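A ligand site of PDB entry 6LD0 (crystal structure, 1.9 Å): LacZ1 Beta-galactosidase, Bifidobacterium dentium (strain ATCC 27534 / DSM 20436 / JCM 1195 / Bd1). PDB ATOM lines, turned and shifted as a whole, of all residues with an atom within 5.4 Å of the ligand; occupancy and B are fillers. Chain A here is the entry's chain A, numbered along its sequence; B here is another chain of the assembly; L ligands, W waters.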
ATOM      1  N   PHE A 154      12.383 -35.442  -1.912  1.00  0.00           N
ATOM      2  CA  PHE A 154      12.789 -34.120  -1.437  1.00  0.00           C
ATOM      3  C   PHE A 154      12.260 -32.932  -2.229  1.00  0.00           C
ATOM      4  O   PHE A 154      12.392 -32.884  -3.454  1.00  0.00           O
ATOM      5  CB  PHE A 154      14.315 -34.047  -1.443  1.00  0.00           C
ATOM      6  CG  PHE A 154      14.919 -33.765  -0.112  1.00  0.00           C
ATOM      7  CD1 PHE A 154      14.402 -34.341   1.024  1.00  0.00           C
ATOM      8  CD2 PHE A 154      16.019 -32.939  -0.013  1.00  0.00           C
ATOM      9  CE1 PHE A 154      14.956 -34.088   2.257  1.00  0.00           C
ATOM     10  CE2 PHE A 154      16.587 -32.687   1.220  1.00  0.00           C
ATOM     11  CZ  PHE A 154      16.055 -33.261   2.355  1.00  0.00           C
ATOM     12  N   MET A 155      11.662 -31.984  -1.503  1.00  0.00           N
ATOM     13  CA  MET A 155      11.102 -30.767  -2.084  1.00  0.00           C
ATOM     14  C   MET A 155      10.184 -31.231  -3.194  1.00  0.00           C
ATOM     15  O   MET A 155      10.254 -30.767  -4.333  1.00  0.00           O
ATOM     16  CB  MET A 155      12.211 -29.858  -2.606  1.00  0.00           C
ATOM     17  CG  MET A 155      13.216 -29.411  -1.526  1.00  0.00           C
ATOM     18  SD  MET A 155      12.656 -28.158  -0.372  1.00  0.00           S
ATOM     19  CE  MET A 155      14.217 -27.366   0.034  1.00  0.00           C
ATOM     20  N   ASP A 181      18.754 -34.751  -1.613  1.00  0.00           N
ATOM     21  CA  ASP A 181      18.680 -34.072  -2.909  1.00  0.00           C
ATOM     22  C   ASP A 181      19.842 -34.432  -3.830  1.00  0.00           C
ATOM     23  O   ASP A 181      20.566 -33.565  -4.289  1.00  0.00           O
ATOM     24  CB  ASP A 181      18.631 -32.557  -2.710  1.00  0.00           C
ATOM     25  CG  ASP A 181      18.398 -31.812  -4.008  1.00  0.00           C
ATOM     26  OD1 ASP A 181      17.540 -32.254  -4.815  1.00  0.00           O
ATOM     27  OD2 ASP A 181      19.097 -30.810  -4.251  1.00  0.00           O
ATOM     28  N   PHE A 182      20.036 -35.722  -4.074  1.00  0.00           N
ATOM     29  CA  PHE A 182      20.968 -36.164  -5.100  1.00  0.00           C
ATOM     30  C   PHE A 182      20.506 -37.540  -5.550  1.00  0.00           C
ATOM     31  O   PHE A 182      19.965 -38.302  -4.753  1.00  0.00           O
ATOM     32  CB  PHE A 182      22.424 -36.179  -4.604  1.00  0.00           C
ATOM     33  CG  PHE A 182      22.672 -37.026  -3.387  1.00  0.00           C
ATOM     34  CD1 PHE A 182      22.973 -38.381  -3.507  1.00  0.00           C
ATOM     35  CD2 PHE A 182      22.637 -36.463  -2.120  1.00  0.00           C
ATOM     36  CE1 PHE A 182      23.213 -39.147  -2.381  1.00  0.00           C
ATOM     37  CE2 PHE A 182      22.871 -37.222  -0.998  1.00  0.00           C
ATOM     38  CZ  PHE A 182      23.158 -38.579  -1.128  1.00  0.00           C
ATOM     39  N   HIS A 381      30.052 -33.125  -5.049  1.00  0.00           N
ATOM     40  CA  HIS A 381      29.416 -34.422  -5.157  1.00  0.00           C
ATOM     41  C   HIS A 381      30.330 -35.260  -6.005  1.00  0.00           C
ATOM     42  O   HIS A 381      31.040 -34.717  -6.853  1.00  0.00           O
ATOM     43  CB  HIS A 381      28.018 -34.339  -5.788  1.00  0.00           C
ATOM     44  CG  HIS A 381      26.898 -34.396  -4.806  1.00  0.00           C
ATOM     45  ND1 HIS A 381      26.637 -35.505  -4.031  1.00  0.00           N
ATOM     46  CD2 HIS A 381      25.949 -33.475  -4.476  1.00  0.00           C
ATOM     47  CE1 HIS A 381      25.595 -35.267  -3.262  1.00  0.00           C
ATOM     48  NE2 HIS A 381      25.156 -34.049  -3.518  1.00  0.00           N
ATOM     49  N   HIS A 415      27.575 -35.962   0.202  1.00  0.00           N
ATOM     50  CA  HIS A 415      27.128 -36.194   1.575  1.00  0.00           C
ATOM     51  C   HIS A 415      27.472 -37.629   1.962  1.00  0.00           C
ATOM     52  O   HIS A 415      26.608 -38.381   2.394  1.00  0.00           O
ATOM     53  CB  HIS A 415      25.609 -35.992   1.689  1.00  0.00           C
ATOM     54  CG  HIS A 415      25.162 -34.599   1.395  1.00  0.00           C
ATOM     55  ND1 HIS A 415      25.559 -33.515   2.141  1.00  0.00           N
ATOM     56  CD2 HIS A 415      24.336 -34.116   0.432  1.00  0.00           C
ATOM     57  CE1 HIS A 415      24.998 -32.416   1.653  1.00  0.00           C
ATOM     58  NE2 HIS A 415      24.250 -32.765   0.621  1.00  0.00           N
ATOM     59  N   ASN A 480      24.364 -34.467   7.745  1.00  0.00           N
ATOM     60  CA  ASN A 480      23.930 -33.286   7.004  1.00  0.00           C
ATOM     61  C   ASN A 480      22.424 -33.027   7.153  1.00  0.00           C
ATOM     62  O   ASN A 480      21.596 -33.869   6.792  1.00  0.00           O
ATOM     63  CB  ASN A 480      24.266 -33.412   5.514  1.00  0.00           C
ATOM     64  CG  ASN A 480      23.874 -32.182   4.728  1.00  0.00           C
ATOM     65  OD1 ASN A 480      24.548 -31.150   4.791  1.00  0.00           O
ATOM     66  ND2 ASN A 480      22.783 -32.278   3.977  1.00  0.00           N
ATOM     67  N   GLU A 481      22.112 -31.852   7.694  1.00  0.00           N
ATOM     68  CA  GLU A 481      20.733 -31.378   7.852  1.00  0.00           C
ATOM     69  C   GLU A 481      19.763 -32.354   8.523  1.00  0.00           C
ATOM     70  O   GLU A 481      18.664 -32.590   8.000  1.00  0.00           O
ATOM     71  CB  GLU A 481      20.188 -30.942   6.490  1.00  0.00           C
ATOM     72  CG  GLU A 481      21.007 -29.824   5.845  1.00  0.00           C
ATOM     73  CD  GLU A 481      20.411 -29.345   4.529  1.00  0.00           C
ATOM     74  OE1 GLU A 481      19.639 -30.099   3.909  1.00  0.00           O
ATOM     75  OE2 GLU A 481      20.721 -28.198   4.126  1.00  0.00           O
ATOM     76  N   GLN A 521      18.695 -24.999   7.565  1.00  0.00           N
ATOM     77  CA  GLN A 521      18.036 -23.744   7.896  1.00  0.00           C
ATOM     78  C   GLN A 521      16.814 -23.994   8.768  1.00  0.00           C
ATOM     79  O   GLN A 521      15.774 -24.407   8.267  1.00  0.00           O
ATOM     80  CB  GLN A 521      17.637 -23.016   6.614  1.00  0.00           C
ATOM     81  CG  GLN A 521      16.898 -21.708   6.837  1.00  0.00           C
ATOM     82  CD  GLN A 521      17.477 -20.583   6.015  1.00  0.00           C
ATOM     83  OE1 GLN A 521      17.872 -20.772   4.867  1.00  0.00           O
ATOM     84  NE2 GLN A 521      17.559 -19.395   6.609  1.00  0.00           N
ATOM     85  N   ASN A 539      23.926 -24.247   6.878  1.00  0.00           N
ATOM     86  CA  ASN A 539      23.408 -24.210   5.517  1.00  0.00           C
ATOM     87  C   ASN A 539      22.285 -23.193   5.463  1.00  0.00           C
ATOM     88  O   ASN A 539      21.250 -23.397   6.099  1.00  0.00           O
ATOM     89  CB  ASN A 539      22.879 -25.589   5.105  1.00  0.00           C
ATOM     90  CG  ASN A 539      23.968 -26.634   4.954  1.00  0.00           C
ATOM     91  OD1 ASN A 539      25.149 -26.345   5.147  1.00  0.00           O
ATOM     92  ND2 ASN A 539      23.560 -27.862   4.647  1.00  0.00           N
ATOM     93  N   TYR A 541      19.883 -20.333   3.073  1.00  0.00           N
ATOM     94  CA  TYR A 541      19.416 -19.981   1.746  1.00  0.00           C
ATOM     95  C   TYR A 541      18.480 -18.783   1.792  1.00  0.00           C
ATOM     96  O   TYR A 541      17.454 -18.750   1.107  1.00  0.00           O
ATOM     97  CB  TYR A 541      18.725 -21.194   1.097  1.00  0.00           C
ATOM     98  CG  TYR A 541      19.680 -22.305   0.737  1.00  0.00           C
ATOM     99  CD1 TYR A 541      20.053 -23.266   1.674  1.00  0.00           C
ATOM    100  CD2 TYR A 541      20.206 -22.399  -0.540  1.00  0.00           C
ATOM    101  CE1 TYR A 541      20.925 -24.286   1.340  1.00  0.00           C
ATOM    102  CE2 TYR A 541      21.086 -23.416  -0.885  1.00  0.00           C
ATOM    103  CZ  TYR A 541      21.431 -24.356   0.064  1.00  0.00           C
ATOM    104  OH  TYR A 541      22.298 -25.372  -0.282  1.00  0.00           O
ATOM    105  N   TYR A 545      15.229 -19.869  -0.958  1.00  0.00           N
ATOM    106  CA  TYR A 545      14.083 -20.652  -0.492  1.00  0.00           C
ATOM    107  C   TYR A 545      13.151 -19.830   0.392  1.00  0.00           C
ATOM    108  O   TYR A 545      12.010 -20.226   0.652  1.00  0.00           O
ATOM    109  CB  TYR A 545      14.554 -21.906   0.265  1.00  0.00           C
ATOM    110  CG  TYR A 545      15.105 -22.975  -0.656  1.00  0.00           C
ATOM    111  CD1 TYR A 545      14.334 -23.486  -1.688  1.00  0.00           C
ATOM    112  CD2 TYR A 545      16.392 -23.459  -0.488  1.00  0.00           C
ATOM    113  CE1 TYR A 545      14.826 -24.463  -2.527  1.00  0.00           C
ATOM    114  CE2 TYR A 545      16.899 -24.441  -1.336  1.00  0.00           C
ATOM    115  CZ  TYR A 545      16.113 -24.931  -2.355  1.00  0.00           C
ATOM    116  OH  TYR A 545      16.592 -25.910  -3.205  1.00  0.00           O
ATOM    117  N   ASN A 546      13.627 -18.679   0.846  1.00  0.00           N
ATOM    118  CA  ASN A 546      12.802 -17.728   1.566  1.00  0.00           C
ATOM    119  C   ASN A 546      13.199 -16.325   1.145  1.00  0.00           C
ATOM    120  O   ASN A 546      14.301 -16.140   0.626  1.00  0.00           O
ATOM    121  CB  ASN A 546      12.943 -17.906   3.077  1.00  0.00           C
ATOM    122  CG  ASN A 546      14.364 -17.688   3.564  1.00  0.00           C
ATOM    123  OD1 ASN A 546      14.897 -16.583   3.498  1.00  0.00           O
ATOM    124  ND2 ASN A 546      14.991 -18.754   4.056  1.00  0.00           N
ATOM    125  N   GLU A 576      26.747 -24.527   3.224  1.00  0.00           N
ATOM    126  CA  GLU A 576      25.908 -24.377   2.025  1.00  0.00           C
ATOM    127  C   GLU A 576      25.272 -23.003   1.936  1.00  0.00           C
ATOM    128  O   GLU A 576      24.746 -22.487   2.931  1.00  0.00           O
ATOM    129  CB  GLU A 576      24.783 -25.427   1.991  1.00  0.00           C
ATOM    130  CG  GLU A 576      25.221 -26.861   1.780  1.00  0.00           C
ATOM    131  CD  GLU A 576      24.039 -27.800   1.661  1.00  0.00           C
ATOM    132  OE1 GLU A 576      22.908 -27.314   1.429  1.00  0.00           O
ATOM    133  OE2 GLU A 576      24.234 -29.026   1.851  1.00  0.00           O
ATOM    134  N   TRP A 621      27.220 -23.847  -1.954  1.00  0.00           N
ATOM    135  CA  TRP A 621      26.571 -24.968  -2.610  1.00  0.00           C
ATOM    136  C   TRP A 621      26.223 -24.529  -4.023  1.00  0.00           C
ATOM    137  O   TRP A 621      25.483 -23.552  -4.163  1.00  0.00           O
ATOM    138  CB  TRP A 621      25.327 -25.372  -1.825  1.00  0.00           C
ATOM    139  CG  TRP A 621      24.769 -26.707  -2.200  1.00  0.00           C
ATOM    140  CD1 TRP A 621      23.597 -26.956  -2.872  1.00  0.00           C
ATOM    141  CD2 TRP A 621      25.336 -27.990  -1.903  1.00  0.00           C
ATOM    142  NE1 TRP A 621      23.417 -28.306  -3.015  1.00  0.00           N
ATOM    143  CE2 TRP A 621      24.464 -28.963  -2.423  1.00  0.00           C
ATOM    144  CE3 TRP A 621      26.490 -28.407  -1.238  1.00  0.00           C
ATOM    145  CZ2 TRP A 621      24.715 -30.328  -2.321  1.00  0.00           C
ATOM    146  CZ3 TRP A 621      26.735 -29.762  -1.128  1.00  0.00           C
ATOM    147  CH2 TRP A 621      25.859 -30.705  -1.670  1.00  0.00           C
ATOM    148  N   PHE A 626      24.649 -31.049 -10.562  1.00  0.00           N
ATOM    149  CA  PHE A 626      24.663 -32.488 -10.386  1.00  0.00           C
ATOM    150  C   PHE A 626      23.267 -33.094 -10.527  1.00  0.00           C
ATOM    151  O   PHE A 626      22.263 -32.376 -10.438  1.00  0.00           O
ATOM    152  CB  PHE A 626      25.282 -32.856  -9.022  1.00  0.00           C
ATOM    153  CG  PHE A 626      24.543 -32.304  -7.841  1.00  0.00           C
ATOM    154  CD1 PHE A 626      24.893 -31.084  -7.282  1.00  0.00           C
ATOM    155  CD2 PHE A 626      23.496 -33.017  -7.255  1.00  0.00           C
ATOM    156  CE1 PHE A 626      24.228 -30.578  -6.176  1.00  0.00           C
ATOM    157  CE2 PHE A 626      22.819 -32.514  -6.160  1.00  0.00           C
ATOM    158  CZ  PHE A 626      23.183 -31.298  -5.608  1.00  0.00           C
ATOM    159  N   ARG A 634      13.756 -28.958  -9.968  1.00  0.00           N
ATOM    160  CA  ARG A 634      15.036 -29.499 -10.417  1.00  0.00           C
ATOM    161  C   ARG A 634      15.119 -29.517 -11.941  1.00  0.00           C
ATOM    162  O   ARG A 634      14.611 -30.426 -12.596  1.00  0.00           O
ATOM    163  CB  ARG A 634      15.257 -30.910  -9.835  1.00  0.00           C
ATOM    164  CG  ARG A 634      15.452 -30.895  -8.312  1.00  0.00           C
ATOM    165  CD  ARG A 634      16.777 -30.232  -7.973  1.00  0.00           C
ATOM    166  NE  ARG A 634      16.964 -29.994  -6.549  1.00  0.00           N
ATOM    167  CZ  ARG A 634      16.820 -28.806  -5.969  1.00  0.00           C
ATOM    168  NH1 ARG A 634      16.477 -27.746  -6.694  1.00  0.00           N
ATOM    169  NH2 ARG A 634      17.004 -28.673  -4.657  1.00  0.00           N
ATOM    170  N   ASN A 638      20.150 -30.510  -9.896  1.00  0.00           N
ATOM    171  CA  ASN A 638      20.401 -29.352  -9.057  1.00  0.00           C
ATOM    172  C   ASN A 638      21.345 -28.406  -9.782  1.00  0.00           C
ATOM    173  O   ASN A 638      22.456 -28.782 -10.140  1.00  0.00           O
ATOM    174  CB  ASN A 638      20.996 -29.807  -7.717  1.00  0.00           C
ATOM    175  CG  ASN A 638      21.110 -28.664  -6.713  1.00  0.00           C
ATOM    176  OD1 ASN A 638      21.741 -27.648  -6.976  1.00  0.00           O
ATOM    177  ND2 ASN A 638      20.506 -28.854  -5.545  1.00  0.00           N
ATOM    178  N   LYS A 640      22.594 -25.403  -8.713  1.00  0.00           N
ATOM    179  CA  LYS A 640      23.258 -24.436  -7.845  1.00  0.00           C
ATOM    180  C   LYS A 640      24.780 -24.414  -8.004  1.00  0.00           C
ATOM    181  O   LYS A 640      25.476 -23.663  -7.324  1.00  0.00           O
ATOM    182  CB  LYS A 640      22.893 -24.695  -6.373  1.00  0.00           C
ATOM    183  CG  LYS A 640      21.446 -24.363  -6.033  1.00  0.00           C
ATOM    184  CD  LYS A 640      21.205 -24.396  -4.524  1.00  0.00           C
ATOM    185  CE  LYS A 640      19.725 -24.188  -4.207  1.00  0.00           C
ATOM    186  NZ  LYS A 640      18.884 -25.335  -4.634  1.00  0.00           N
ATOM    187  N   ASN B 159      10.266 -19.775   4.785  1.00  0.00           N
ATOM    188  CA  ASN B 159      10.636 -20.523   5.977  1.00  0.00           C
ATOM    189  C   ASN B 159      10.170 -19.734   7.201  1.00  0.00           C
ATOM    190  O   ASN B 159      10.974 -19.329   8.038  1.00  0.00           O
ATOM    191  CB  ASN B 159      12.151 -20.765   6.056  1.00  0.00           C
ATOM    192  CG  ASN B 159      12.723 -21.389   4.794  1.00  0.00           C
ATOM    193  OD1 ASN B 159      13.820 -21.035   4.355  1.00  0.00           O
ATOM    194  ND2 ASN B 159      12.000 -22.337   4.212  1.00  0.00           N
HETATM  195  C1  LIG L   1      19.524 -27.847  -2.027  1.00  0.00           C
HETATM  196  C2  LIG L   1      20.346 -28.449  -0.929  1.00  0.00           C
HETATM  197  C3  LIG L   1      20.683 -29.910  -1.222  1.00  0.00           C
HETATM  198  O1  LIG L   1      21.131 -30.102  -2.566  1.00  0.00           O
HETATM  199  C4  LIG L   1      21.750 -30.357  -0.224  1.00  0.00           C
HETATM  200  O2  LIG L   1      22.101 -31.720  -0.443  1.00  0.00           O
HETATM  201  C5  LIG L   1      21.235 -30.203   1.214  1.00  0.00           C
HETATM  202  C6  LIG L   1      19.604 -28.446   0.397  1.00  0.00           C
HETATM  203  C7  LIG L   1      19.081 -27.067   0.801  1.00  0.00           C
HETATM  204  C8  LIG L   1      17.830 -27.202   1.673  1.00  0.00           C
HETATM  205  N1  LIG L   1      20.508 -28.965   1.409  1.00  0.00           N
HETATM  206  O3  LIG L   1      20.061 -27.180  -2.907  1.00  0.00           O
HETATM  207  O4  LIG L   1      18.202 -28.021  -2.067  1.00  0.00           O
HETATM  208  C9  LIG L   1      17.450 -25.892   2.354  1.00  0.00           C
HETATM  209  C10 LIG L   1      16.101 -25.999   3.062  1.00  0.00           C
HETATM  210  C11 LIG L   1      15.858 -24.796   3.968  1.00  0.00           C
HETATM  211  C12 LIG L   1      16.029 -23.492   3.216  1.00  0.00           C
HETATM  212  O   HOH W   1      19.963 -32.655   3.206  1.00  0.00           O
HETATM  213  O   HOH W   2      19.314 -25.503   5.026  1.00  0.00           O
HETATM  214  O   HOH W   3      22.679 -33.099  -2.368  1.00  0.00           O
HETATM  215  O   HOH W   4      20.107 -33.530   0.327  1.00  0.00           O
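ND2 of Asn 638 lies within hydrogen-bond range of O3 of the ligand, 3.2 Å away.
NE1 of Trp 621 sits at hydrogen-bond distance from O1 of the ligand (2.9 Å).
The guanidinium group (NH2) of Arg 634 lies within salt-bridge range of an oxygen (O4) of the ligand (2.9 Å).
O3 of the ligand lies within salt-bridge range of NZ of Lys 640.
The side-chain carboxylate of Asp 181 lies within hydrogen-bond range of an oxygen (O1) of the ligand, at 2.7 Å.
OE1 of Glu 576 lies within salt-bridge range of N1 of the ligand.
OH of Tyr 545 sits at hydrogen-bond distance from O4 of the ligand.
The side-chain carboxylate (OE2) of Glu 481 lies within salt-bridge range of a nitrogen (N1) of the ligand, 2.8 Å away.
NE2 of His 415 sits at hydrogen-bond distance from O2 of the ligand (2.6 Å).
The side-chain amide nitrogen of Asn 539 lies within hydrogen-bond range of the side-chain amide oxygen of Asn 480, 3.4 Å away.
The side-chain amide oxygen of Gln 521 lies within hydrogen-bond range of the backbone NH of Tyr 541 (2.7 Å).
The backbone NH (N) of Gln 521 is in hydrogen-bond range of the backbone carbonyl oxygen (O) of Asn 539.
The side-chain amino group of Lys 640 lies within hydrogen-bond range of the side-chain hydroxyl of Tyr 545, at 2.8 Å.
The side-chain carboxylate (OD1) of Asp 181 is in salt-bridge range of the guanidinium group (NE) of Arg 634 (2.9 Å).
The guanidinium group (NH2) of Arg 634 is in hydrogen-bond range of the side-chain hydroxyl (OH) of Tyr 545 (3.1 Å).
ND2 of Asn 546 lies within hydrogen-bond range of OD1 of Asn 159 of chain B (2.6 Å).
The side-chain amide oxygen of Asn 539 sits at hydrogen-bond distance from the backbone NH of Glu 576, 3.1 Å away.
CE of Met 155 touches C10 of the ligand (3.8 Å).
Asn 480 touches the ligand (ND2 to C5, 3.8 Å).
CB of Gln 521 touches C11 of the ligand, 3.7 Å away.
Tyr 541 touches the ligand.
CZ of Phe 626 touches O1 of the ligand, 3.9 Å away.
OD1 of Asn 159 of chain B touches C12 of the ligand, 3.5 Å away.
Within 4 Å of the ligand: Met 155, Asp 181, His 415, Asn 480, Glu 481, Gln 521, Tyr 541, Tyr 545, Glu 576, Trp 621, Phe 626, Arg 634, Asn 638, Lys 640 and Asn 159 of chain B.
Water W3 lies within hydrogen-bond range of O2 of the ligand (2.4 Å), NE2 of His 381 (2.9 Å), O of Asp 181 (2.9 Å) and NE2 of His 415 (3.4 Å).
Water W4 lies within hydrogen-bond range of the backbone NH (N) of Asp 181 (2.7 Å) and an oxygen (O2) of the ligand (2.8 Å).
Water W2 lies within hydrogen-bond range of N of Gln 521 (2.7 Å), O of Asn 539 (3.1 Å) and OE2 of Glu 481 (3.2 Å).
Water W1 lies within hydrogen-bond range of the side-chain carboxylate (OE1) of Glu 481 (2.7 Å) and the side-chain amide nitrogen (ND2) of Asn 480 (2.9 Å).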
